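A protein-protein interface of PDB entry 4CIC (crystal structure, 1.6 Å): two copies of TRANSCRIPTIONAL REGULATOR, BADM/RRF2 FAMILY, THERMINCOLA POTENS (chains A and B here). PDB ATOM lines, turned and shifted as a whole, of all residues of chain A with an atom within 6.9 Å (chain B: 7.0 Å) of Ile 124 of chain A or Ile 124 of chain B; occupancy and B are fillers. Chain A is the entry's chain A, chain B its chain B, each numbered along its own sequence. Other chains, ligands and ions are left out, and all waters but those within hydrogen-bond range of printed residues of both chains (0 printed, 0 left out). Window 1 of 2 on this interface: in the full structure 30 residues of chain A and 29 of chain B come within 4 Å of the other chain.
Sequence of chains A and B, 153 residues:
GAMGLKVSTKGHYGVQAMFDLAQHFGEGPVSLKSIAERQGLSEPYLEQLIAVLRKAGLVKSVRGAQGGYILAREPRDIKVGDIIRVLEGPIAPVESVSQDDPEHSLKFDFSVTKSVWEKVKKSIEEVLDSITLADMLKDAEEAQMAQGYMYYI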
ATOM      1  N   MET A   3     -27.505 -27.597  -2.390  1.00  0.00           N
ATOM      2  CA  MET A   3     -26.168 -27.482  -1.827  1.00  0.00           C
ATOM      3  C   MET A   3     -25.476 -28.835  -1.956  1.00  0.00           C
ATOM      4  O   MET A   3     -24.282 -28.964  -1.697  1.00  0.00           O
ATOM      5  CB  MET A   3     -26.271 -27.090  -0.351  1.00  0.00           C
ATOM      6  CG  MET A   3     -25.344 -25.976   0.106  1.00  0.00           C
ATOM      7  SD  MET A   3     -25.615 -24.401  -0.727  1.00  0.00           S
ATOM      8  CE  MET A   3     -27.406 -24.315  -0.728  1.00  0.00           C
ATOM      9  N   LEU A   5     -25.921 -31.675  -0.188  1.00  0.00           N
ATOM     10  CA  LEU A   5     -25.621 -32.429   1.026  1.00  0.00           C
ATOM     11  C   LEU A   5     -26.015 -33.881   0.820  1.00  0.00           C
ATOM     12  O   LEU A   5     -27.104 -34.165   0.342  1.00  0.00           O
ATOM     13  CB  LEU A   5     -26.387 -31.867   2.220  1.00  0.00           C
ATOM     14  CG  LEU A   5     -26.381 -32.767   3.466  1.00  0.00           C
ATOM     15  CD1 LEU A   5     -25.024 -32.722   4.142  1.00  0.00           C
ATOM     16  CD2 LEU A   5     -27.496 -32.406   4.445  1.00  0.00           C
ATOM     17  N   GLY A  81     -27.482 -35.507  17.632  1.00  0.00           N
ATOM     18  CA  GLY A  81     -26.039 -35.351  17.566  1.00  0.00           C
ATOM     19  C   GLY A  81     -25.240 -36.375  18.370  1.00  0.00           C
ATOM     20  O   GLY A  81     -24.118 -36.720  17.984  1.00  0.00           O
ATOM     21  N   LYS A 119     -17.592 -23.078   9.899  1.00  0.00           N
ATOM     22  CA  LYS A 119     -18.875 -22.456  10.211  1.00  0.00           C
ATOM     23  C   LYS A 119     -20.040 -23.346   9.797  1.00  0.00           C
ATOM     24  O   LYS A 119     -21.047 -23.435  10.517  1.00  0.00           O
ATOM     25  CB  LYS A 119     -18.991 -21.078   9.552  1.00  0.00           C
ATOM     26  CG  LYS A 119     -18.300 -19.984  10.336  1.00  0.00           C
ATOM     27  CD  LYS A 119     -18.091 -18.745   9.489  1.00  0.00           C
ATOM     28  CE  LYS A 119     -17.238 -17.725  10.218  1.00  0.00           C
ATOM     29  NZ  LYS A 119     -16.947 -16.550   9.356  1.00  0.00           N
ATOM     30  N   VAL A 120     -19.909 -24.001   8.646  1.00  0.00           N
ATOM     31  CA  VAL A 120     -20.902 -24.999   8.235  1.00  0.00           C
ATOM     32  C   VAL A 120     -20.993 -26.111   9.274  1.00  0.00           C
ATOM     33  O   VAL A 120     -22.094 -26.502   9.685  1.00  0.00           O
ATOM     34  CB  VAL A 120     -20.566 -25.598   6.865  1.00  0.00           C
ATOM     35  CG1 VAL A 120     -21.526 -26.715   6.501  1.00  0.00           C
ATOM     36  CG2 VAL A 120     -20.611 -24.497   5.792  1.00  0.00           C
ATOM     37  N   LYS A 121     -19.841 -26.614   9.701  1.00  0.00           N
ATOM     38  CA  LYS A 121     -19.816 -27.717  10.682  1.00  0.00           C
ATOM     39  C   LYS A 121     -20.496 -27.320  11.984  1.00  0.00           C
ATOM     40  O   LYS A 121     -21.271 -28.092  12.568  1.00  0.00           O
ATOM     41  CB  LYS A 121     -18.368 -28.113  10.971  1.00  0.00           C
ATOM     42  CG  LYS A 121     -18.220 -29.152  12.081  1.00  0.00           C
ATOM     43  CD  LYS A 121     -16.764 -29.214  12.544  1.00  0.00           C
ATOM     44  CE  LYS A 121     -16.566 -30.190  13.688  1.00  0.00           C
ATOM     45  NZ  LYS A 121     -15.135 -30.238  14.099  1.00  0.00           N
ATOM     46  N   LYS A 122     -20.204 -26.111  12.437  1.00  0.00           N
ATOM     47  CA  LYS A 122     -20.751 -25.636  13.698  1.00  0.00           C
ATOM     48  C   LYS A 122     -22.269 -25.548  13.631  1.00  0.00           C
ATOM     49  O   LYS A 122     -22.956 -25.909  14.602  1.00  0.00           O
ATOM     50  CB  LYS A 122     -20.134 -24.278  14.049  1.00  0.00           C
ATOM     51  CG  LYS A 122     -19.756 -24.143  15.507  1.00  0.00           C
ATOM     52  CD  LYS A 122     -18.786 -25.225  15.939  1.00  0.00           C
ATOM     53  CE  LYS A 122     -18.584 -25.178  17.445  1.00  0.00           C
ATOM     54  NZ  LYS A 122     -19.894 -25.107  18.166  1.00  0.00           N
ATOM     55  N   SER A 123     -22.794 -25.116  12.484  1.00  0.00           N
ATOM     56  CA  SER A 123     -24.235 -24.929  12.346  1.00  0.00           C
ATOM     57  C   SER A 123     -24.934 -26.282  12.325  1.00  0.00           C
ATOM     58  O   SER A 123     -26.014 -26.426  12.900  1.00  0.00           O
ATOM     59  CB  SER A 123     -24.597 -24.152  11.084  1.00  0.00           C
ATOM     60  OG  SER A 123     -24.480 -24.968   9.927  1.00  0.00           O
ATOM     61  N   ILE A 124     -24.324 -27.259  11.658  1.00  0.00           N
ATOM     62  CA  ILE A 124     -24.850 -28.634  11.668  1.00  0.00           C
ATOM     63  C   ILE A 124     -24.866 -29.218  13.082  1.00  0.00           C
ATOM     64  O   ILE A 124     -25.870 -29.834  13.522  1.00  0.00           O
ATOM     65  CB  ILE A 124     -24.021 -29.560  10.768  1.00  0.00           C
ATOM     66  CG1 ILE A 124     -24.111 -29.100   9.310  1.00  0.00           C
ATOM     67  CG2 ILE A 124     -24.467 -31.029  10.943  1.00  0.00           C
ATOM     68  CD1 ILE A 124     -23.182 -29.880   8.384  1.00  0.00           C
ATOM     69  N   GLU A 125     -23.756 -29.037  13.798  1.00  0.00           N
ATOM     70  CA  GLU A 125     -23.663 -29.487  15.184  1.00  0.00           C
ATOM     71  C   GLU A 125     -24.742 -28.831  16.032  1.00  0.00           C
ATOM     72  O   GLU A 125     -25.368 -29.493  16.890  1.00  0.00           O
ATOM     73  CB  GLU A 125     -22.275 -29.203  15.762  1.00  0.00           C
ATOM     74  CG  GLU A 125     -22.099 -29.671  17.208  1.00  0.00           C
ATOM     75  CD  GLU A 125     -20.738 -29.286  17.776  1.00  0.00           C
ATOM     76  OE1 GLU A 125     -20.020 -28.502  17.115  1.00  0.00           O
ATOM     77  OE2 GLU A 125     -20.389 -29.764  18.877  1.00  0.00           O
ATOM     78  N   GLU A 126     -25.006 -27.550  15.780  1.00  0.00           N
ATOM     79  CA  GLU A 126     -26.043 -26.868  16.549  1.00  0.00           C
ATOM     80  C   GLU A 126     -27.441 -27.437  16.281  1.00  0.00           C
ATOM     81  O   GLU A 126     -28.215 -27.645  17.225  1.00  0.00           O
ATOM     82  CB  GLU A 126     -26.033 -25.357  16.321  1.00  0.00           C
ATOM     83  CG  GLU A 126     -26.482 -24.590  17.566  1.00  0.00           C
ATOM     84  CD  GLU A 126     -27.394 -23.409  17.267  1.00  0.00           C
ATOM     85  OE1 GLU A 126     -27.470 -22.980  16.096  1.00  0.00           O
ATOM     86  OE2 GLU A 126     -28.039 -22.909  18.216  1.00  0.00           O
ATOM     87  N   VAL A 127     -27.772 -27.682  15.013  1.00  0.00           N
ATOM     88  CA  VAL A 127     -29.081 -28.252  14.691  1.00  0.00           C
ATOM     89  C   VAL A 127     -29.228 -29.618  15.334  1.00  0.00           C
ATOM     90  O   VAL A 127     -30.234 -29.880  16.016  1.00  0.00           O
ATOM     91  CB  VAL A 127     -29.313 -28.400  13.168  1.00  0.00           C
ATOM     92  CG1 VAL A 127     -30.610 -29.170  12.893  1.00  0.00           C
ATOM     93  CG2 VAL A 127     -29.357 -27.026  12.500  1.00  0.00           C
ATOM     94  N   LEU A 128     -28.224 -30.477  15.173  1.00  0.00           N
ATOM     95  CA  LEU A 128     -28.381 -31.866  15.633  1.00  0.00           C
ATOM     96  C   LEU A 128     -28.354 -31.983  17.154  1.00  0.00           C
ATOM     97  O   LEU A 128     -28.878 -32.947  17.730  1.00  0.00           O
ATOM     98  CB  LEU A 128     -27.357 -32.797  14.999  1.00  0.00           C
ATOM     99  CG  LEU A 128     -27.455 -32.891  13.463  1.00  0.00           C
ATOM    100  CD1 LEU A 128     -26.383 -33.790  12.921  1.00  0.00           C
ATOM    101  CD2 LEU A 128     -28.842 -33.395  13.067  1.00  0.00           C
ATOM    102  N   ASP A 129     -27.759 -31.002  17.818  1.00  0.00           N
ATOM    103  CA  ASP A 129     -27.795 -31.004  19.275  1.00  0.00           C
ATOM    104  C   ASP A 129     -29.089 -30.395  19.802  1.00  0.00           C
ATOM    105  O   ASP A 129     -29.398 -30.524  20.981  1.00  0.00           O
ATOM    106  CB  ASP A 129     -26.578 -30.263  19.839  1.00  0.00           C
ATOM    107  CG  ASP A 129     -25.323 -31.117  19.820  1.00  0.00           C
ATOM    108  OD1 ASP A 129     -25.436 -32.346  19.580  1.00  0.00           O
ATOM    109  OD2 ASP A 129     -24.230 -30.564  20.071  1.00  0.00           O
ATOM    110  N   SER A 130     -29.841 -29.734  18.928  1.00  0.00           N
ATOM    111  CA  SER A 130     -31.053 -29.041  19.349  1.00  0.00           C
ATOM    112  C   SER A 130     -32.268 -29.943  19.256  1.00  0.00           C
ATOM    113  O   SER A 130     -33.356 -29.553  19.666  1.00  0.00           O
ATOM    114  CB  SER A 130     -31.291 -27.800  18.491  1.00  0.00           C
ATOM    115  OG  SER A 130     -31.791 -28.158  17.212  1.00  0.00           O
ATOM    116  N   MET B   3     -19.309 -34.467  13.997  1.00  0.00           N
ATOM    117  CA  MET B   3     -20.414 -34.969  13.193  1.00  0.00           C
ATOM    118  C   MET B   3     -19.888 -35.716  11.970  1.00  0.00           C
ATOM    119  O   MET B   3     -20.642 -36.389  11.285  1.00  0.00           O
ATOM    120  CB  MET B   3     -21.304 -33.818  12.715  1.00  0.00           C
ATOM    121  CG  MET B   3     -21.877 -32.933  13.811  1.00  0.00           C
ATOM    122  SD  MET B   3     -23.169 -33.745  14.757  1.00  0.00           S
ATOM    123  CE  MET B   3     -22.328 -34.015  16.310  1.00  0.00           C
ATOM    124  N   LEU B   5     -18.588 -34.349   9.125  1.00  0.00           N
ATOM    125  CA  LEU B   5     -18.866 -33.680   7.856  1.00  0.00           C
ATOM    126  C   LEU B   5     -17.626 -33.774   6.985  1.00  0.00           C
ATOM    127  O   LEU B   5     -16.527 -33.541   7.459  1.00  0.00           O
ATOM    128  CB  LEU B   5     -19.191 -32.205   8.080  1.00  0.00           C
ATOM    129  CG  LEU B   5     -19.200 -31.351   6.800  1.00  0.00           C
ATOM    130  CD1 LEU B   5     -20.500 -31.571   6.044  1.00  0.00           C
ATOM    131  CD2 LEU B   5     -18.982 -29.876   7.101  1.00  0.00           C
ATOM    132  N   GLY B  81     -22.637 -19.814  -1.216  1.00  0.00           N
ATOM    133  CA  GLY B  81     -23.718 -20.671  -1.675  1.00  0.00           C
ATOM    134  C   GLY B  81     -23.948 -20.663  -3.183  1.00  0.00           C
ATOM    135  O   GLY B  81     -24.325 -21.696  -3.741  1.00  0.00           O
ATOM    136  N   TRP B 117     -32.898 -34.197   8.548  1.00  0.00           N
ATOM    137  CA  TRP B 117     -31.855 -33.872   7.565  1.00  0.00           C
ATOM    138  C   TRP B 117     -32.227 -32.637   6.770  1.00  0.00           C
ATOM    139  O   TRP B 117     -31.350 -31.894   6.357  1.00  0.00           O
ATOM    140  CB  TRP B 117     -31.550 -35.019   6.597  1.00  0.00           C
ATOM    141  CG  TRP B 117     -31.280 -36.325   7.261  1.00  0.00           C
ATOM    142  CD1 TRP B 117     -31.831 -37.523   6.925  1.00  0.00           C
ATOM    143  CD2 TRP B 117     -30.402 -36.581   8.365  1.00  0.00           C
ATOM    144  NE1 TRP B 117     -31.360 -38.515   7.754  1.00  0.00           N
ATOM    145  CE2 TRP B 117     -30.505 -37.962   8.666  1.00  0.00           C
ATOM    146  CE3 TRP B 117     -29.571 -35.783   9.150  1.00  0.00           C
ATOM    147  CZ2 TRP B 117     -29.767 -38.564   9.682  1.00  0.00           C
ATOM    148  CZ3 TRP B 117     -28.851 -36.384  10.177  1.00  0.00           C
ATOM    149  CH2 TRP B 117     -28.959 -37.762  10.432  1.00  0.00           C
ATOM    150  N   LYS B 119     -33.681 -30.097   7.962  1.00  0.00           N
ATOM    151  CA  LYS B 119     -33.289 -28.999   8.845  1.00  0.00           C
ATOM    152  C   LYS B 119     -31.782 -28.761   8.801  1.00  0.00           C
ATOM    153  O   LYS B 119     -31.328 -27.604   8.815  1.00  0.00           O
ATOM    154  CB  LYS B 119     -33.751 -29.259  10.279  1.00  0.00           C
ATOM    155  CG  LYS B 119     -35.246 -29.134  10.472  1.00  0.00           C
ATOM    156  CD  LYS B 119     -35.607 -29.534  11.888  1.00  0.00           C
ATOM    157  CE  LYS B 119     -37.095 -29.461  12.141  1.00  0.00           C
ATOM    158  NZ  LYS B 119     -37.380 -29.805  13.560  1.00  0.00           N
ATOM    159  N   VAL B 120     -31.004 -29.839   8.733  1.00  0.00           N
ATOM    160  CA  VAL B 120     -29.549 -29.714   8.547  1.00  0.00           C
ATOM    161  C   VAL B 120     -29.250 -29.003   7.232  1.00  0.00           C
ATOM    162  O   VAL B 120     -28.424 -28.066   7.182  1.00  0.00           O
ATOM    163  CB  VAL B 120     -28.853 -31.090   8.578  1.00  0.00           C
ATOM    164  CG1 VAL B 120     -27.385 -30.980   8.182  1.00  0.00           C
ATOM    165  CG2 VAL B 120     -28.968 -31.699   9.997  1.00  0.00           C
ATOM    166  N   LYS B 121     -29.930 -29.422   6.171  1.00  0.00           N
ATOM    167  CA  LYS B 121     -29.683 -28.820   4.853  1.00  0.00           C
ATOM    168  C   LYS B 121     -29.979 -27.323   4.869  1.00  0.00           C
ATOM    169  O   LYS B 121     -29.226 -26.508   4.305  1.00  0.00           O
ATOM    170  CB  LYS B 121     -30.526 -29.505   3.780  1.00  0.00           C
ATOM    171  CG  LYS B 121     -30.448 -28.793   2.420  1.00  0.00           C
ATOM    172  CD  LYS B 121     -31.555 -29.280   1.486  1.00  0.00           C
ATOM    173  CE  LYS B 121     -32.931 -29.054   2.094  1.00  0.00           C
ATOM    174  NZ  LYS B 121     -34.009 -29.591   1.223  1.00  0.00           N
ATOM    175  N   LYS B 122     -31.078 -26.961   5.513  1.00  0.00           N
ATOM    176  CA  LYS B 122     -31.479 -25.562   5.629  1.00  0.00           C
ATOM    177  C   LYS B 122     -30.421 -24.717   6.302  1.00  0.00           C
ATOM    178  O   LYS B 122     -30.095 -23.619   5.822  1.00  0.00           O
ATOM    179  CB  LYS B 122     -32.770 -25.474   6.437  1.00  0.00           C
ATOM    180  CG  LYS B 122     -33.891 -24.770   5.722  1.00  0.00           C
ATOM    181  CD  LYS B 122     -34.173 -25.411   4.383  1.00  0.00           C
ATOM    182  CE  LYS B 122     -35.059 -24.503   3.558  1.00  0.00           C
ATOM    183  NZ  LYS B 122     -34.577 -23.090   3.637  1.00  0.00           N
ATOM    184  N   SER B 123     -29.872 -25.223   7.401  1.00  0.00           N
ATOM    185  CA  SER B 123     -28.910 -24.448   8.172  1.00  0.00           C
ATOM    186  C   SER B 123     -27.618 -24.267   7.377  1.00  0.00           C
ATOM    187  O   SER B 123     -27.008 -23.201   7.449  1.00  0.00           O
ATOM    188  CB  SER B 123     -28.593 -25.084   9.519  1.00  0.00           C
ATOM    189  OG  SER B 123     -27.668 -26.146   9.369  1.00  0.00           O
ATOM    190  N   ILE B 124     -27.202 -25.296   6.634  1.00  0.00           N
ATOM    191  CA  ILE B 124     -26.018 -25.155   5.767  1.00  0.00           C
ATOM    192  C   ILE B 124     -26.245 -24.088   4.697  1.00  0.00           C
ATOM    193  O   ILE B 124     -25.379 -23.213   4.458  1.00  0.00           O
ATOM    194  CB  ILE B 124     -25.658 -26.465   5.063  1.00  0.00           C
ATOM    195  CG1 ILE B 124     -25.256 -27.527   6.096  1.00  0.00           C
ATOM    196  CG2 ILE B 124     -24.556 -26.230   4.017  1.00  0.00           C
ATOM    197  CD1 ILE B 124     -25.159 -28.943   5.507  1.00  0.00           C
ATOM    198  N   GLU B 125     -27.407 -24.159   4.049  1.00  0.00           N
ATOM    199  CA  GLU B 125     -27.794 -23.187   3.026  1.00  0.00           C
ATOM    200  C   GLU B 125     -27.767 -21.783   3.607  1.00  0.00           C
ATOM    201  O   GLU B 125     -27.279 -20.830   2.965  1.00  0.00           O
ATOM    202  CB  GLU B 125     -29.175 -23.521   2.458  1.00  0.00           C
ATOM    203  CG  GLU B 125     -29.698 -22.537   1.407  1.00  0.00           C
ATOM    204  CD  GLU B 125     -31.069 -22.946   0.875  1.00  0.00           C
ATOM    205  OE1 GLU B 125     -31.493 -24.095   1.143  1.00  0.00           O
ATOM    206  OE2 GLU B 125     -31.724 -22.119   0.203  1.00  0.00           O
ATOM    207  N   GLU B 126     -28.243 -21.648   4.840  1.00  0.00           N
ATOM    208  CA  GLU B 126     -28.252 -20.330   5.477  1.00  0.00           C
ATOM    209  C   GLU B 126     -26.850 -19.794   5.761  1.00  0.00           C
ATOM    210  O   GLU B 126     -26.589 -18.600   5.562  1.00  0.00           O
ATOM    211  CB  GLU B 126     -29.081 -20.346   6.757  1.00  0.00           C
ATOM    212  CG  GLU B 126     -30.571 -20.470   6.505  1.00  0.00           C
ATOM    213  CD  GLU B 126     -31.376 -20.576   7.786  1.00  0.00           C
ATOM    214  OE1 GLU B 126     -30.914 -20.064   8.828  1.00  0.00           O
ATOM    215  OE2 GLU B 126     -32.470 -21.176   7.751  1.00  0.00           O
ATOM    216  N   VAL B 127     -25.957 -20.659   6.240  1.00  0.00           N
ATOM    217  CA  VAL B 127     -24.583 -20.231   6.489  1.00  0.00           C
ATOM    218  C   VAL B 127     -23.953 -19.838   5.173  1.00  0.00           C
ATOM    219  O   VAL B 127     -23.385 -18.739   5.054  1.00  0.00           O
ATOM    220  CB  VAL B 127     -23.718 -21.342   7.133  1.00  0.00           C
ATOM    221  CG1 VAL B 127     -22.248 -20.918   7.151  1.00  0.00           C
ATOM    222  CG2 VAL B 127     -24.195 -21.632   8.549  1.00  0.00           C
ATOM    223  N   LEU B 128     -24.066 -20.699   4.165  1.00  0.00           N
ATOM    224  CA  LEU B 128     -23.354 -20.396   2.905  1.00  0.00           C
ATOM    225  C   LEU B 128     -23.927 -19.208   2.133  1.00  0.00           C
ATOM    226  O   LEU B 128     -23.217 -18.562   1.347  1.00  0.00           O
ATOM    227  CB  LEU B 128     -23.262 -21.627   2.011  1.00  0.00           C
ATOM    228  CG  LEU B 128     -22.492 -22.799   2.661  1.00  0.00           C
ATOM    229  CD1 LEU B 128     -22.429 -23.983   1.744  1.00  0.00           C
ATOM    230  CD2 LEU B 128     -21.090 -22.362   3.065  1.00  0.00           C
ATOM    231  N   ASP B 129     -25.201 -18.905   2.348  1.00  0.00           N
ATOM    232  CA  ASP B 129     -25.778 -17.725   1.708  1.00  0.00           C
ATOM    233  C   ASP B 129     -25.478 -16.445   2.481  1.00  0.00           C
ATOM    234  O   ASP B 129     -25.732 -15.349   1.990  1.00  0.00           O
ATOM    235  CB  ASP B 129     -27.291 -17.906   1.548  1.00  0.00           C
ATOM    236  CG  ASP B 129     -27.646 -18.774   0.351  1.00  0.00           C
ATOM    237  OD1 ASP B 129     -26.729 -19.095  -0.445  1.00  0.00           O
ATOM    238  OD2 ASP B 129     -28.841 -19.116   0.199  1.00  0.00           O
ATOM    239  N   SER B 130     -24.950 -16.585   3.693  1.00  0.00           N
ATOM    240  CA  SER B 130     -24.703 -15.424   4.540  1.00  0.00           C
ATOM    241  C   SER B 130     -23.283 -14.919   4.392  1.00  0.00           C
ATOM    242  O   SER B 130     -22.930 -13.912   4.989  1.00  0.00           O
ATOM    243  CB  SER B 130     -24.960 -15.756   6.012  1.00  0.00           C
ATOM    244  OG  SER B 130     -23.896 -16.532   6.551  1.00  0.00           O
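Met 3 of chain A touches Ile 124 of chain B (CG to CG2, 3.998 Å).
Met 3 of chain A touches Glu 125 of chain B.
Leu 128 of chain B touches Met 3 of chain A.
Met 3 of chain B touches Gly 81 of chain A (CE to O, 3.7 Å).
Ile 124 of chain B touches Val 120 of chain A (CG1 to CG1, 3.8 Å).
CG2 of Val 127 of chain B touches CB of Ser 123 of chain A (3.6 Å).
Ile 124 of chain A touches Leu 5 of chain B (CD1 to CD1, 3.9 Å).
Val 120 of chain B touches Ile 124 of chain A (CG1 to CG1, 3.9 Å).
Ile 124 of chain A touches Ile 124 of chain B.
CD2 of Leu 128 of chain A touches CG2 of Val 120 of chain B (3.5 Å).
O of Val 127 of chain A lies within hydrogen-bond range of OG of Ser 130 of chain A (2.6 Å).
N of Gly 81 of chain B lies within hydrogen-bond range of O of Leu 128 of chain B, at 2.9 Å.
The backbone carbonyl oxygen (O) of Val 127 of chain B lies within hydrogen-bond range of the side-chain hydroxyl (OG) of Ser 130 of chain B (2.7 Å).
The backbone carbonyl oxygen of Val 120 of chain B sits at hydrogen-bond distance from the side-chain hydroxyl of Ser 123 of chain B.
The backbone carbonyl oxygen (O) of Val 120 of chain A is in hydrogen-bond range of the side-chain hydroxyl (OG) of Ser 123 of chain A (2.8 Å).
The backbone NH (N) of Gly 81 of chain A sits at hydrogen-bond distance from the backbone carbonyl oxygen (O) of Leu 128 of chain A (2.9 Å).
Of the printed residues of chain B, Gly 81 of chain A touches Met 3 (3.7 Å).
Of the printed residues of chain B, Ile 124 of chain A touches Leu 5 (3.9 Å), Val 120 (3.9 Å) and Ile 124 (3.6 Å).
Printed residues of chain B within 4 Å of Val 127 of chain A: Ser 123 (3.6 Å).
Of the printed residues of chain B, Leu 128 of chain A touches Met 3 (3.7 Å) and Val 120 (3.5 Å).
Gly 81 of chain B touches none of the printed residues of chain A.
Printed residues of chain A within 4 Å of Ser 123 of chain B: Ser 123 (3.4 Å) and Val 127 (3.6 Å).
Printed residues of chain A within 4 Å of Ile 124 of chain B: Met 3, Val 120 and Ile 124.
Of the printed residues of chain A, Leu 128 of chain B touches Met 3 and Val 120.
The nearest residue of chain B that does not touch Ile 124 of chain A is Ser 123 of chain B (4.2 Å).
The nearest printed residue of chain A that does not touch Ile 124 of chain B is Leu 5 of chain A (4.02 Å).
Hydrophobic or aromatic side chains of chain A within 4 Å of the printed part of chain B: Met 3, Val 120, Ile 124, Val 127 and Leu 128.
Hydrophobic or aromatic side chains of chain B within 4 Å of the printed part of chain A: Met 3, Leu 5, Val 120, Ile 124, Val 127 and Leu 128.
The side-chain hydroxyl (OG) of Ser 123 of chain A sits at hydrogen-bond distance from the side-chain hydroxyl (OG) of Ser 123 of chain B, 3.4 Å away.
Met 3 of chain A touches Ile 124 of chain B, but with the chains exchanged Ile 124 of chain A does not touch Met 3 of chain B (4.3 Å).
Met 3 of chain A touches Leu 128 of chain B, and with the chains exchanged Leu 128 of chain A touches Met 3 of chain B.
Val 120 of chain A touches Leu 128 of chain B, and with the chains exchanged Leu 128 of chain A touches Val 120 of chain B.
Ser 123 of chain A touches Val 127 of chain B, and with the chains exchanged Val 127 of chain A touches Ser 123 of chain B.
Positions printed for both chains: 3, 5, 81, 119, 120, 121, 122, 123, 124, 125, 126, 127, 128, 129 and 130.
Of the 14 pairs that touch across the chains among the printed residues, 10 have their exchanged pair printed and touching as well.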
